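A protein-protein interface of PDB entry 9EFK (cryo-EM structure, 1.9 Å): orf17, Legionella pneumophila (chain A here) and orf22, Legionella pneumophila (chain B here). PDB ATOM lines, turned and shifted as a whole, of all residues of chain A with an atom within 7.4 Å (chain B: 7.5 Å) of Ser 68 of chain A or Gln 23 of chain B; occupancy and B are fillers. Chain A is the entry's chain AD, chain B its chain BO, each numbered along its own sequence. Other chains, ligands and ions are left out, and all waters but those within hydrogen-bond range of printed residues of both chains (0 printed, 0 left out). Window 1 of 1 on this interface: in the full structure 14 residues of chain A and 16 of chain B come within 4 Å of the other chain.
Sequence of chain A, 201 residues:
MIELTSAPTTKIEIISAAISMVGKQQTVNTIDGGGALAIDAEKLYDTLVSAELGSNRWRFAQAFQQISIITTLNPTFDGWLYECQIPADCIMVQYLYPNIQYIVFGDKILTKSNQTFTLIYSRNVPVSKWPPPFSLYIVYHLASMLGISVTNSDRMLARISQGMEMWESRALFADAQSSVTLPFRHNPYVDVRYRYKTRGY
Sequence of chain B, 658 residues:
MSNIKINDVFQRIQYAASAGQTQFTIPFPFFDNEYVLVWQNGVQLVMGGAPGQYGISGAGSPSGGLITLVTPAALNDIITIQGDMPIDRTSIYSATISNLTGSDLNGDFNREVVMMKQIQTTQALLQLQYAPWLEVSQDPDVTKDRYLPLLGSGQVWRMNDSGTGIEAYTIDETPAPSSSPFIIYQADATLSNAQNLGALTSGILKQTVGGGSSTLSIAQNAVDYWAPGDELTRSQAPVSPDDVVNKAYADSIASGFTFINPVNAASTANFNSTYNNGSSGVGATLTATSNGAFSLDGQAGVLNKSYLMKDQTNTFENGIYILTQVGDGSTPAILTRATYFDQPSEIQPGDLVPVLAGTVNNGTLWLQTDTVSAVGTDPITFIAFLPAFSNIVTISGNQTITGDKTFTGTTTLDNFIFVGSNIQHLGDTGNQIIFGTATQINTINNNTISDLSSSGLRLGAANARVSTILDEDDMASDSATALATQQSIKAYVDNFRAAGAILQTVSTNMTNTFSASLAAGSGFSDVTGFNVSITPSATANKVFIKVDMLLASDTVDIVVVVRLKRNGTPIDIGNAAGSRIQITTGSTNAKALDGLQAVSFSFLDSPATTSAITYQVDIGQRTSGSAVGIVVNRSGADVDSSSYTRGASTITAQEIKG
Of the printed residues of chain B, Ser 68 of chain A touches Tyr 15, Gln 21, Gln 23 and Phe 24.
Of chain A, only Gln 65 (3.7 Å), Gln 66 (3.1 Å) and Ser 68 (3.6 Å) come within 4 Å of Gln 23 of chain B.
Printed residues of chain B within 4 Å of Ile 69 of chain A: Tyr 15 (3.2 Å) and Ala 16 (2.8 Å).
Of the printed residues of chain A, Phe 24 of chain B touches Ser 68 (3.5 Å).
Of the printed residues of chain A, Tyr 15 of chain B touches Ser 68 (3.5 Å), Ile 69 (3.2 Å), Thr 71 (3.6 Å) and Gln 85 (3.5 Å).
Of the printed residues of chain B, Pro 87 of chain A touches Thr 25 (3.5 Å).
The nearest residue of chain A that does not touch Gln 23 of chain B is Phe 64 of chain A (5.2 Å).
The nearest printed residue of chain A that does not touch Thr 22 of chain B is Ser 68 of chain A (7.2 Å).
O of Phe 117 of chain A is in hydrogen-bond range of N of Ile 67 of chain A (2.9 Å).
The backbone NH of Ser 18 of chain B sits at hydrogen-bond distance from the side-chain amide oxygen of Gln 21 of chain B, at 3.2 Å.
The backbone NH (N) of Ile 70 of chain A lies within hydrogen-bond range of the backbone carbonyl oxygen (O) of Glu 83 of chain A.
Printed residues of chain A that touch a printed residue of chain B: Gln 65, Gln 66, Ile 67, Ser 68, Ile 69, Ile 70, Thr 71, Gln 85, Ile 86 and Pro 87.
Hydrophobic or aromatic side chains of chain B within 4 Å of the printed part of chain A: Tyr 15, Ala 16, Phe 24 and Leu 66.
Among the printed residues, 20 pairs touch across the chains.
Among the printed residues, no Asp or Glu carboxylate lies within 4 Å of a Lys or Arg side-chain nitrogen of the other chain.
OE1 of Gln 65 of chain A touches CD1 of Leu 66 of chain B, 3.6 Å away.
Gln 66 of chain A touches Gln 21 of chain B.
Tyr 15 of chain B touches Ser 68 of chain A.
Ser 68 of chain A touches Gln 23 of chain B (OG to O, 3.6 Å).
Ser 68 of chain A touches Phe 24 of chain B.
O of Ile 69 of chain A touches CA of Tyr 15 of chain B (3.2 Å).
Thr 71 of chain A touches Tyr 15 of chain B.
Pro 87 of chain A touches Thr 25 of chain B (CA to OG1, 3.5 Å).
The side-chain amide nitrogen (NE2) of Gln 21 of chain B sits at hydrogen-bond distance from the side-chain hydroxyl (OG) of Ser 68 of chain A.
The backbone NH (N) of Gln 66 of chain A sits at hydrogen-bond distance from the side-chain amide oxygen (OE1) of Gln 23 of chain B.
The backbone NH (N) of Ala 16 of chain B is in hydrogen-bond range of the backbone carbonyl oxygen (O) of Ile 69 of chain A.
The side-chain hydroxyl (OG1) of Thr 71 of chain A lies within hydrogen-bond range of the side-chain amide oxygen (OE1) of Gln 14 of chain B (2.9 Å).
The side-chain hydroxyl (OG1) of Thr 25 of chain B is in hydrogen-bond range of the side-chain amide nitrogen (NE2) of Gln 65 of chain A, at 2.9 Å.
The side-chain amide nitrogen of Gln 21 of chain B is in hydrogen-bond range of the backbone carbonyl oxygen of Ile 67 of chain A, at 3.4 Å.
N of Thr 22 of chain B sits at hydrogen-bond distance from OE1 of Gln 66 of chain A (3.0 Å).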
ATOM      1  N   PHE A  64      -3.170  20.202   0.902  1.00  0.00           N
ATOM      2  CA  PHE A  64      -3.110  18.970   0.133  1.00  0.00           C
ATOM      3  C   PHE A  64      -4.474  18.297   0.126  1.00  0.00           C
ATOM      4  O   PHE A  64      -5.307  18.526   1.003  1.00  0.00           O
ATOM      5  CB  PHE A  64      -2.029  18.020   0.664  1.00  0.00           C
ATOM      6  CG  PHE A  64      -2.305  17.469   2.029  1.00  0.00           C
ATOM      7  CD1 PHE A  64      -1.989  18.193   3.161  1.00  0.00           C
ATOM      8  CD2 PHE A  64      -2.849  16.208   2.181  1.00  0.00           C
ATOM      9  CE1 PHE A  64      -2.232  17.681   4.412  1.00  0.00           C
ATOM     10  CE2 PHE A  64      -3.092  15.692   3.430  1.00  0.00           C
ATOM     11  CZ  PHE A  64      -2.782  16.427   4.548  1.00  0.00           C
ATOM     12  N   GLN A  65      -4.691  17.468  -0.893  1.00  0.00           N
ATOM     13  CA  GLN A  65      -5.945  16.751  -1.070  1.00  0.00           C
ATOM     14  C   GLN A  65      -5.736  15.636  -2.081  1.00  0.00           C
ATOM     15  O   GLN A  65      -4.864  15.725  -2.945  1.00  0.00           O
ATOM     16  CB  GLN A  65      -7.063  17.687  -1.538  1.00  0.00           C
ATOM     17  CG  GLN A  65      -8.448  17.085  -1.454  1.00  0.00           C
ATOM     18  CD  GLN A  65      -9.456  17.825  -2.293  1.00  0.00           C
ATOM     19  OE1 GLN A  65      -9.920  18.898  -1.924  1.00  0.00           O
ATOM     20  NE2 GLN A  65      -9.805  17.250  -3.433  1.00  0.00           N
ATOM     21  N   GLN A  66      -6.544  14.587  -1.967  1.00  0.00           N
ATOM     22  CA  GLN A  66      -6.511  13.505  -2.939  1.00  0.00           C
ATOM     23  C   GLN A  66      -7.122  13.950  -4.263  1.00  0.00           C
ATOM     24  O   GLN A  66      -8.010  14.802  -4.310  1.00  0.00           O
ATOM     25  CB  GLN A  66      -7.250  12.284  -2.399  1.00  0.00           C
ATOM     26  CG  GLN A  66      -6.631  11.703  -1.143  1.00  0.00           C
ATOM     27  CD  GLN A  66      -7.461  10.596  -0.534  1.00  0.00           C
ATOM     28  OE1 GLN A  66      -8.657  10.497  -0.780  1.00  0.00           O
ATOM     29  NE2 GLN A  66      -6.827   9.755   0.267  1.00  0.00           N
ATOM     30  N   ILE A  67      -6.641  13.354  -5.346  1.00  0.00           N
ATOM     31  CA  ILE A  67      -7.085  13.667  -6.700  1.00  0.00           C
ATOM     32  C   ILE A  67      -7.956  12.526  -7.211  1.00  0.00           C
ATOM     33  O   ILE A  67      -7.758  11.363  -6.850  1.00  0.00           O
ATOM     34  CB  ILE A  67      -5.873  13.904  -7.623  1.00  0.00           C
ATOM     35  CG1 ILE A  67      -4.987  14.991  -7.043  1.00  0.00           C
ATOM     36  CG2 ILE A  67      -6.312  14.374  -8.960  1.00  0.00           C
ATOM     37  CD1 ILE A  67      -5.721  16.272  -6.832  1.00  0.00           C
ATOM     38  N   SER A  68      -8.929  12.864  -8.055  1.00  0.00           N
ATOM     39  CA  SER A  68      -9.924  11.913  -8.538  1.00  0.00           C
ATOM     40  C   SER A  68      -9.811  11.748 -10.045  1.00  0.00           C
ATOM     41  O   SER A  68      -9.751  12.738 -10.775  1.00  0.00           O
ATOM     42  CB  SER A  68     -11.336  12.369  -8.175  1.00  0.00           C
ATOM     43  OG  SER A  68     -11.450  12.649  -6.796  1.00  0.00           O
ATOM     44  N   ILE A  69      -9.811  10.501 -10.506  1.00  0.00           N
ATOM     45  CA  ILE A  69      -9.784  10.200 -11.932  1.00  0.00           C
ATOM     46  C   ILE A  69     -11.174  10.416 -12.519  1.00  0.00           C
ATOM     47  O   ILE A  69     -12.170   9.934 -11.974  1.00  0.00           O
ATOM     48  CB  ILE A  69      -9.300   8.763 -12.170  1.00  0.00           C
ATOM     49  CG1 ILE A  69      -7.831   8.629 -11.780  1.00  0.00           C
ATOM     50  CG2 ILE A  69      -9.502   8.353 -13.610  1.00  0.00           C
ATOM     51  CD1 ILE A  69      -7.304   7.238 -11.912  1.00  0.00           C
ATOM     52  N   ILE A  70     -11.243  11.137 -13.631  1.00  0.00           N
ATOM     53  CA  ILE A  70     -12.504  11.430 -14.305  1.00  0.00           C
ATOM     54  C   ILE A  70     -12.796  10.326 -15.311  1.00  0.00           C
ATOM     55  O   ILE A  70     -11.927   9.956 -16.107  1.00  0.00           O
ATOM     56  CB  ILE A  70     -12.445  12.801 -14.997  1.00  0.00           C
ATOM     57  CG1 ILE A  70     -12.145  13.900 -13.982  1.00  0.00           C
ATOM     58  CG2 ILE A  70     -13.742  13.091 -15.717  1.00  0.00           C
ATOM     59  CD1 ILE A  70     -11.767  15.210 -14.604  1.00  0.00           C
ATOM     60  N   THR A  71     -14.017   9.802 -15.284  1.00  0.00           N
ATOM     61  CA  THR A  71     -14.393   8.723 -16.185  1.00  0.00           C
ATOM     62  C   THR A  71     -14.623   9.236 -17.606  1.00  0.00           C
ATOM     63  O   THR A  71     -14.877  10.420 -17.835  1.00  0.00           O
ATOM     64  CB  THR A  71     -15.652   8.012 -15.690  1.00  0.00           C
ATOM     65  OG1 THR A  71     -16.731   8.947 -15.621  1.00  0.00           O
ATOM     66  CG2 THR A  71     -15.425   7.418 -14.322  1.00  0.00           C
ATOM     67  N   GLU A  83      -7.102  11.168 -16.891  1.00  0.00           N
ATOM     68  CA  GLU A  83      -7.281  12.601 -16.711  1.00  0.00           C
ATOM     69  C   GLU A  83      -7.972  12.794 -15.370  1.00  0.00           C
ATOM     70  O   GLU A  83      -9.048  12.236 -15.148  1.00  0.00           O
ATOM     71  CB  GLU A  83      -8.120  13.171 -17.854  1.00  0.00           C
ATOM     72  CG  GLU A  83      -7.754  14.557 -18.297  1.00  0.00           C
ATOM     73  CD  GLU A  83      -8.150  14.828 -19.735  1.00  0.00           C
ATOM     74  OE1 GLU A  83      -8.654  13.902 -20.400  1.00  0.00           O
ATOM     75  OE2 GLU A  83      -7.953  15.968 -20.204  1.00  0.00           O
ATOM     76  N   CYS A  84      -7.361  13.561 -14.474  1.00  0.00           N
ATOM     77  CA  CYS A  84      -7.875  13.653 -13.117  1.00  0.00           C
ATOM     78  C   CYS A  84      -8.082  15.107 -12.710  1.00  0.00           C
ATOM     79  O   CYS A  84      -7.408  16.013 -13.199  1.00  0.00           O
ATOM     80  CB  CYS A  84      -6.960  12.923 -12.121  1.00  0.00           C
ATOM     81  SG  CYS A  84      -5.252  13.412 -12.093  1.00  0.00           S
ATOM     82  N   GLN A  85      -9.037  15.305 -11.806  1.00  0.00           N
ATOM     83  CA  GLN A  85      -9.562  16.621 -11.471  1.00  0.00           C
ATOM     84  C   GLN A  85      -8.714  17.313 -10.414  1.00  0.00           C
ATOM     85  O   GLN A  85      -8.336  16.715  -9.407  1.00  0.00           O
ATOM     86  CB  GLN A  85     -11.002  16.498 -10.973  1.00  0.00           C
ATOM     87  CG  GLN A  85     -11.612  17.790 -10.470  1.00  0.00           C
ATOM     88  CD  GLN A  85     -12.196  18.635 -11.576  1.00  0.00           C
ATOM     89  OE1 GLN A  85     -12.718  18.117 -12.556  1.00  0.00           O
ATOM     90  NE2 GLN A  85     -12.110  19.946 -11.423  1.00  0.00           N
ATOM     91  N   ILE A  86      -8.432  18.588 -10.652  1.00  0.00           N
ATOM     92  CA  ILE A  86      -7.704  19.450  -9.724  1.00  0.00           C
ATOM     93  C   ILE A  86      -8.661  19.924  -8.633  1.00  0.00           C
ATOM     94  O   ILE A  86      -9.840  20.172  -8.921  1.00  0.00           O
ATOM     95  CB  ILE A  86      -7.058  20.615 -10.493  1.00  0.00           C
ATOM     96  CG1 ILE A  86      -5.986  20.080 -11.441  1.00  0.00           C
ATOM     97  CG2 ILE A  86      -6.456  21.639  -9.570  1.00  0.00           C
ATOM     98  CD1 ILE A  86      -5.384  21.128 -12.339  1.00  0.00           C
ATOM     99  N   PRO A  87      -8.214  20.059  -7.382  1.00  0.00           N
ATOM    100  CA  PRO A  87      -9.118  20.490  -6.309  1.00  0.00           C
ATOM    101  C   PRO A  87      -9.725  21.861  -6.561  1.00  0.00           C
ATOM    102  O   PRO A  87      -9.144  22.711  -7.236  1.00  0.00           O
ATOM    103  CB  PRO A  87      -8.210  20.512  -5.076  1.00  0.00           C
ATOM    104  CG  PRO A  87      -7.185  19.512  -5.370  1.00  0.00           C
ATOM    105  CD  PRO A  87      -6.930  19.588  -6.842  1.00  0.00           C
ATOM    106  N   LYS A 108      -6.305  19.854 -16.075  1.00  0.00           N
ATOM    107  CA  LYS A 108      -6.291  18.507 -15.535  1.00  0.00           C
ATOM    108  C   LYS A 108      -4.864  18.102 -15.201  1.00  0.00           C
ATOM    109  O   LYS A 108      -3.898  18.777 -15.556  1.00  0.00           O
ATOM    110  CB  LYS A 108      -6.893  17.512 -16.530  1.00  0.00           C
ATOM    111  CG  LYS A 108      -8.248  17.904 -17.064  1.00  0.00           C
ATOM    112  CD  LYS A 108      -9.313  17.810 -15.997  1.00  0.00           C
ATOM    113  CE  LYS A 108     -10.653  18.268 -16.535  1.00  0.00           C
ATOM    114  NZ  LYS A 108     -10.983  17.577 -17.804  1.00  0.00           N
ATOM    115  N   ILE A 109      -4.745  16.976 -14.511  1.00  0.00           N
ATOM    116  CA  ILE A 109      -3.472  16.311 -14.282  1.00  0.00           C
ATOM    117  C   ILE A 109      -3.541  14.960 -14.975  1.00  0.00           C
ATOM    118  O   ILE A 109      -4.528  14.234 -14.828  1.00  0.00           O
ATOM    119  CB  ILE A 109      -3.176  16.160 -12.779  1.00  0.00           C
ATOM    120  CG1 ILE A 109      -2.929  17.530 -12.150  1.00  0.00           C
ATOM    121  CG2 ILE A 109      -1.999  15.233 -12.543  1.00  0.00           C
ATOM    122  CD1 ILE A 109      -2.907  17.516 -10.652  1.00  0.00           C
ATOM    123  N   PHE A 117      -3.401   9.416  -5.532  1.00  0.00           N
ATOM    124  CA  PHE A 117      -2.463  10.524  -5.619  1.00  0.00           C
ATOM    125  C   PHE A 117      -2.948  11.675  -4.756  1.00  0.00           C
ATOM    126  O   PHE A 117      -4.151  11.930  -4.663  1.00  0.00           O
ATOM    127  CB  PHE A 117      -2.296  11.008  -7.059  1.00  0.00           C
ATOM    128  CG  PHE A 117      -1.831   9.949  -8.004  1.00  0.00           C
ATOM    129  CD1 PHE A 117      -0.555   9.439  -7.916  1.00  0.00           C
ATOM    130  CD2 PHE A 117      -2.668   9.474  -8.993  1.00  0.00           C
ATOM    131  CE1 PHE A 117      -0.129   8.464  -8.789  1.00  0.00           C
ATOM    132  CE2 PHE A 117      -2.243   8.504  -9.868  1.00  0.00           C
ATOM    133  CZ  PHE A 117      -0.972   8.000  -9.767  1.00  0.00           C
ATOM    134  N   THR A 118      -2.007  12.369  -4.129  1.00  0.00           N
ATOM    135  CA  THR A 118      -2.289  13.547  -3.325  1.00  0.00           C
ATOM    136  C   THR A 118      -1.566  14.737  -3.934  1.00  0.00           C
ATOM    137  O   THR A 118      -0.377  14.648  -4.248  1.00  0.00           O
ATOM    138  CB  THR A 118      -1.847  13.343  -1.877  1.00  0.00           C
ATOM    139  OG1 THR A 118      -2.552  12.231  -1.316  1.00  0.00           O
ATOM    140  CG2 THR A 118      -2.132  14.578  -1.053  1.00  0.00           C
ATOM    141  N   ILE B  13     -20.358  15.839 -12.338  1.00  0.00           N
ATOM    142  CA  ILE B  13     -19.029  15.255 -12.459  1.00  0.00           C
ATOM    143  C   ILE B  13     -19.110  13.798 -12.034  1.00  0.00           C
ATOM    144  O   ILE B  13     -19.907  13.429 -11.171  1.00  0.00           O
ATOM    145  CB  ILE B  13     -17.978  16.030 -11.627  1.00  0.00           C
ATOM    146  CG1 ILE B  13     -16.564  15.592 -11.997  1.00  0.00           C
ATOM    147  CG2 ILE B  13     -18.201  15.829 -10.147  1.00  0.00           C
ATOM    148  CD1 ILE B  13     -16.137  16.005 -13.372  1.00  0.00           C
ATOM    149  N   GLN B  14     -18.292  12.962 -12.662  1.00  0.00           N
ATOM    150  CA  GLN B  14     -18.255  11.545 -12.344  1.00  0.00           C
ATOM    151  C   GLN B  14     -16.811  11.081 -12.242  1.00  0.00           C
ATOM    152  O   GLN B  14     -15.976  11.449 -13.068  1.00  0.00           O
ATOM    153  CB  GLN B  14     -19.006  10.725 -13.389  1.00  0.00           C
ATOM    154  CG  GLN B  14     -19.141   9.270 -13.041  1.00  0.00           C
ATOM    155  CD  GLN B  14     -19.977   8.527 -14.042  1.00  0.00           C
ATOM    156  OE1 GLN B  14     -19.492   8.134 -15.097  1.00  0.00           O
ATOM    157  NE2 GLN B  14     -21.247   8.339 -13.724  1.00  0.00           N
ATOM    158  N   TYR B  15     -16.533  10.250 -11.241  1.00  0.00           N
ATOM    159  CA  TYR B  15     -15.180   9.837 -10.904  1.00  0.00           C
ATOM    160  C   TYR B  15     -15.077   8.322 -10.862  1.00  0.00           C
ATOM    161  O   TYR B  15     -16.062   7.621 -10.631  1.00  0.00           O
ATOM    162  CB  TYR B  15     -14.743  10.380  -9.547  1.00  0.00           C
ATOM    163  CG  TYR B  15     -14.641  11.874  -9.461  1.00  0.00           C
ATOM    164  CD1 TYR B  15     -13.958  12.597 -10.422  1.00  0.00           C
ATOM    165  CD2 TYR B  15     -15.225  12.561  -8.412  1.00  0.00           C
ATOM    166  CE1 TYR B  15     -13.860  13.961 -10.335  1.00  0.00           C
ATOM    167  CE2 TYR B  15     -15.134  13.919  -8.320  1.00  0.00           C
ATOM    168  CZ  TYR B  15     -14.453  14.616  -9.282  1.00  0.00           C
ATOM    169  OH  TYR B  15     -14.362  15.976  -9.188  1.00  0.00           O
ATOM    170  N   ALA B  16     -13.867   7.828 -11.091  1.00  0.00           N
ATOM    171  CA  ALA B  16     -13.516   6.430 -10.877  1.00  0.00           C
ATOM    172  C   ALA B  16     -12.533   6.394  -9.717  1.00  0.00           C
ATOM    173  O   ALA B  16     -11.365   6.757  -9.878  1.00  0.00           O
ATOM    174  CB  ALA B  16     -12.917   5.808 -12.133  1.00  0.00           C
ATOM    175  N   ALA B  17     -13.007   5.966  -8.555  1.00  0.00           N
ATOM    176  CA  ALA B  17     -12.214   6.038  -7.339  1.00  0.00           C
ATOM    177  C   ALA B  17     -11.029   5.085  -7.387  1.00  0.00           C
ATOM    178  O   ALA B  17     -11.075   4.027  -8.015  1.00  0.00           O
ATOM    179  CB  ALA B  17     -13.077   5.717  -6.124  1.00  0.00           C
ATOM    180  N   SER B  18      -9.954   5.484  -6.725  1.00  0.00           N
ATOM    181  CA  SER B  18      -8.847   4.585  -6.458  1.00  0.00           C
ATOM    182  C   SER B  18      -9.067   3.901  -5.115  1.00  0.00           C
ATOM    183  O   SER B  18      -9.893   4.324  -4.305  1.00  0.00           O
ATOM    184  CB  SER B  18      -7.520   5.339  -6.465  1.00  0.00           C
ATOM    185  OG  SER B  18      -7.534   6.414  -5.546  1.00  0.00           O
ATOM    186  N   GLY B  20      -9.120   2.979  -1.544  1.00  0.00           N
ATOM    187  CA  GLY B  20      -8.910   3.689  -0.301  1.00  0.00           C
ATOM    188  C   GLY B  20      -9.127   5.185  -0.340  1.00  0.00           C
ATOM    189  O   GLY B  20      -8.849   5.856   0.659  1.00  0.00           O
ATOM    190  N   GLN B  21      -9.618   5.729  -1.447  1.00  0.00           N
ATOM    191  CA  GLN B  21      -9.834   7.164  -1.560  1.00  0.00           C
ATOM    192  C   GLN B  21     -11.114   7.584  -0.849  1.00  0.00           C
ATOM    193  O   GLN B  21     -12.122   6.875  -0.888  1.00  0.00           O
ATOM    194  CB  GLN B  21      -9.896   7.568  -3.031  1.00  0.00           C
ATOM    195  CG  GLN B  21     -10.150   9.037  -3.266  1.00  0.00           C
ATOM    196  CD  GLN B  21     -10.273   9.373  -4.727  1.00  0.00           C
ATOM    197  OE1 GLN B  21     -10.174   8.500  -5.582  1.00  0.00           O
ATOM    198  NE2 GLN B  21     -10.496  10.639  -5.026  1.00  0.00           N
ATOM    199  N   THR B  22     -11.072   8.747  -0.197  1.00  0.00           N
ATOM    200  CA  THR B  22     -12.246   9.305   0.457  1.00  0.00           C
ATOM    201  C   THR B  22     -12.609  10.713   0.008  1.00  0.00           C
ATOM    202  O   THR B  22     -13.762  11.110   0.185  1.00  0.00           O
ATOM    203  CB  THR B  22     -12.069   9.326   1.984  1.00  0.00           C
ATOM    204  OG1 THR B  22     -10.928  10.116   2.331  1.00  0.00           O
ATOM    205  CG2 THR B  22     -11.892   7.925   2.526  1.00  0.00           C
ATOM    206  N   GLN B  23     -11.680  11.473  -0.562  1.00  0.00           N
ATOM    207  CA  GLN B  23     -11.913  12.873  -0.897  1.00  0.00           C
ATOM    208  C   GLN B  23     -12.202  13.009  -2.386  1.00  0.00           C
ATOM    209  O   GLN B  23     -11.385  12.610  -3.218  1.00  0.00           O
ATOM    210  CB  GLN B  23     -10.710  13.726  -0.505  1.00  0.00           C
ATOM    211  CG  GLN B  23     -10.386  13.695   0.971  1.00  0.00           C
ATOM    212  CD  GLN B  23      -9.072  14.369   1.292  1.00  0.00           C
ATOM    213  OE1 GLN B  23      -8.061  14.114   0.649  1.00  0.00           O
ATOM    214  NE2 GLN B  23      -9.083  15.239   2.288  1.00  0.00           N
ATOM    215  N   PHE B  24     -13.358  13.579  -2.717  1.00  0.00           N
ATOM    216  CA  PHE B  24     -13.774  13.782  -4.099  1.00  0.00           C
ATOM    217  C   PHE B  24     -14.190  15.233  -4.281  1.00  0.00           C
ATOM    218  O   PHE B  24     -15.089  15.714  -3.589  1.00  0.00           O
ATOM    219  CB  PHE B  24     -14.919  12.837  -4.470  1.00  0.00           C
ATOM    220  CG  PHE B  24     -14.554  11.389  -4.383  1.00  0.00           C
ATOM    221  CD1 PHE B  24     -14.724  10.687  -3.205  1.00  0.00           C
ATOM    222  CD2 PHE B  24     -14.037  10.729  -5.478  1.00  0.00           C
ATOM    223  CE1 PHE B  24     -14.384   9.361  -3.124  1.00  0.00           C
ATOM    224  CE2 PHE B  24     -13.696   9.402  -5.401  1.00  0.00           C
ATOM    225  CZ  PHE B  24     -13.872   8.717  -4.223  1.00  0.00           C
ATOM    226  N   THR B  25     -13.547  15.920  -5.220  1.00  0.00           N
ATOM    227  CA  THR B  25     -13.795  17.338  -5.435  1.00  0.00           C
ATOM    228  C   THR B  25     -15.179  17.578  -6.023  1.00  0.00           C
ATOM    229  O   THR B  25     -15.635  16.846  -6.901  1.00  0.00           O
ATOM    230  CB  THR B  25     -12.728  17.911  -6.369  1.00  0.00           C
ATOM    231  OG1 THR B  25     -11.465  17.925  -5.699  1.00  0.00           O
ATOM    232  CG2 THR B  25     -13.071  19.321  -6.817  1.00  0.00           C
ATOM    233  N   ILE B  26     -15.853  18.613  -5.532  1.00  0.00           N
ATOM    234  CA  ILE B  26     -17.029  19.171  -6.194  1.00  0.00           C
ATOM    235  C   ILE B  26     -16.548  20.344  -7.043  1.00  0.00           C
ATOM    236  O   ILE B  26     -16.241  21.408  -6.487  1.00  0.00           O
ATOM    237  CB  ILE B  26     -18.094  19.620  -5.187  1.00  0.00           C
ATOM    238  CG1 ILE B  26     -18.411  18.507  -4.193  1.00  0.00           C
ATOM    239  CG2 ILE B  26     -19.360  20.047  -5.909  1.00  0.00           C
ATOM    240  CD1 ILE B  26     -19.409  18.912  -3.141  1.00  0.00           C
ATOM    241  N   LEU B  66     -15.894  19.964  -1.426  1.00  0.00           N
ATOM    242  CA  LEU B  66     -15.310  18.644  -1.252  1.00  0.00           C
ATOM    243  C   LEU B  66     -16.331  17.686  -0.658  1.00  0.00           C
ATOM    244  O   LEU B  66     -17.110  18.062   0.220  1.00  0.00           O
ATOM    245  CB  LEU B  66     -14.078  18.709  -0.344  1.00  0.00           C
ATOM    246  CG  LEU B  66     -13.355  17.389  -0.099  1.00  0.00           C
ATOM    247  CD1 LEU B  66     -12.782  16.866  -1.391  1.00  0.00           C
ATOM    248  CD2 LEU B  66     -12.267  17.557   0.936  1.00  0.00           C
ATOM    249  N   ILE B  67     -16.311  16.446  -1.137  1.00  0.00           N
ATOM    250  CA  ILE B  67     -17.081  15.341  -0.580  1.00  0.00           C
ATOM    251  C   ILE B  67     -16.101  14.384   0.080  1.00  0.00           C
ATOM    252  O   ILE B  67     -15.111  13.981  -0.539  1.00  0.00           O
ATOM    253  CB  ILE B  67     -17.898  14.616  -1.663  1.00  0.00           C
ATOM    254  CG1 ILE B  67     -19.053  15.486  -2.152  1.00  0.00           C
ATOM    255  CG2 ILE B  67     -18.405  13.283  -1.156  1.00  0.00           C
ATOM    256  CD1 ILE B  67     -20.086  15.766  -1.110  1.00  0.00           C
ATOM    257  N   THR B  68     -16.368  14.018   1.331  1.00  0.00           N
ATOM    258  CA  THR B  68     -15.502  13.108   2.076  1.00  0.00           C
ATOM    259  C   THR B  68     -16.308  11.886   2.490  1.00  0.00           C
ATOM    260  O   THR B  68     -17.173  11.976   3.364  1.00  0.00           O
ATOM    261  CB  THR B  68     -14.897  13.795   3.297  1.00  0.00           C
ATOM    262  OG1 THR B  68     -14.160  14.950   2.883  1.00  0.00           O
ATOM    263  CG2 THR B  68     -13.959  12.851   4.017  1.00  0.00           C
ATOM    264  N   LEU B  69     -16.019  10.746   1.873  1.00  0.00           N
ATOM    265  CA  LEU B  69     -16.684   9.506   2.243  1.00  0.00           C
ATOM    266  C   LEU B  69     -16.222   9.037   3.615  1.00  0.00           C
ATOM    267  O   LEU B  69     -15.040   9.121   3.952  1.00  0.00           O
ATOM    268  CB  LEU B  69     -16.403   8.421   1.210  1.00  0.00           C
ATOM    269  CG  LEU B  69     -16.883   8.668  -0.216  1.00  0.00           C
ATOM    270  CD1 LEU B  69     -16.612   7.453  -1.072  1.00  0.00           C
ATOM    271  CD2 LEU B  69     -18.356   9.014  -0.232  1.00  0.00           C
ATOM    272  N   ILE B  79     -18.303   7.379  -8.605  1.00  0.00           N
ATOM    273  CA  ILE B  79     -18.895   8.426  -7.784  1.00  0.00           C
ATOM    274  C   ILE B  79     -19.474   9.479  -8.714  1.00  0.00           C
ATOM    275  O   ILE B  79     -18.771   9.993  -9.588  1.00  0.00           O
ATOM    276  CB  ILE B  79     -17.861   9.054  -6.835  1.00  0.00           C
ATOM    277  CG1 ILE B  79     -17.187   7.981  -5.983  1.00  0.00           C
ATOM    278  CG2 ILE B  79     -18.513  10.101  -5.960  1.00  0.00           C
ATOM    279  CD1 ILE B  79     -18.092   7.361  -4.972  1.00  0.00           C
ATOM    280  N   ILE B  81     -21.608  13.173  -8.817  1.00  0.00           N
ATOM    281  CA  ILE B  81     -22.002  14.356  -8.064  1.00  0.00           C
ATOM    282  C   ILE B  81     -22.737  15.293  -9.010  1.00  0.00           C
ATOM    283  O   ILE B  81     -22.243  15.590 -10.100  1.00  0.00           O
ATOM    284  CB  ILE B  81     -20.785  15.057  -7.435  1.00  0.00           C
ATOM    285  CG1 ILE B  81     -20.034  14.092  -6.520  1.00  0.00           C
ATOM    286  CG2 ILE B  81     -21.211  16.286  -6.670  1.00  0.00           C
ATOM    287  CD1 ILE B  81     -18.644  14.543  -6.169  1.00  0.00           C
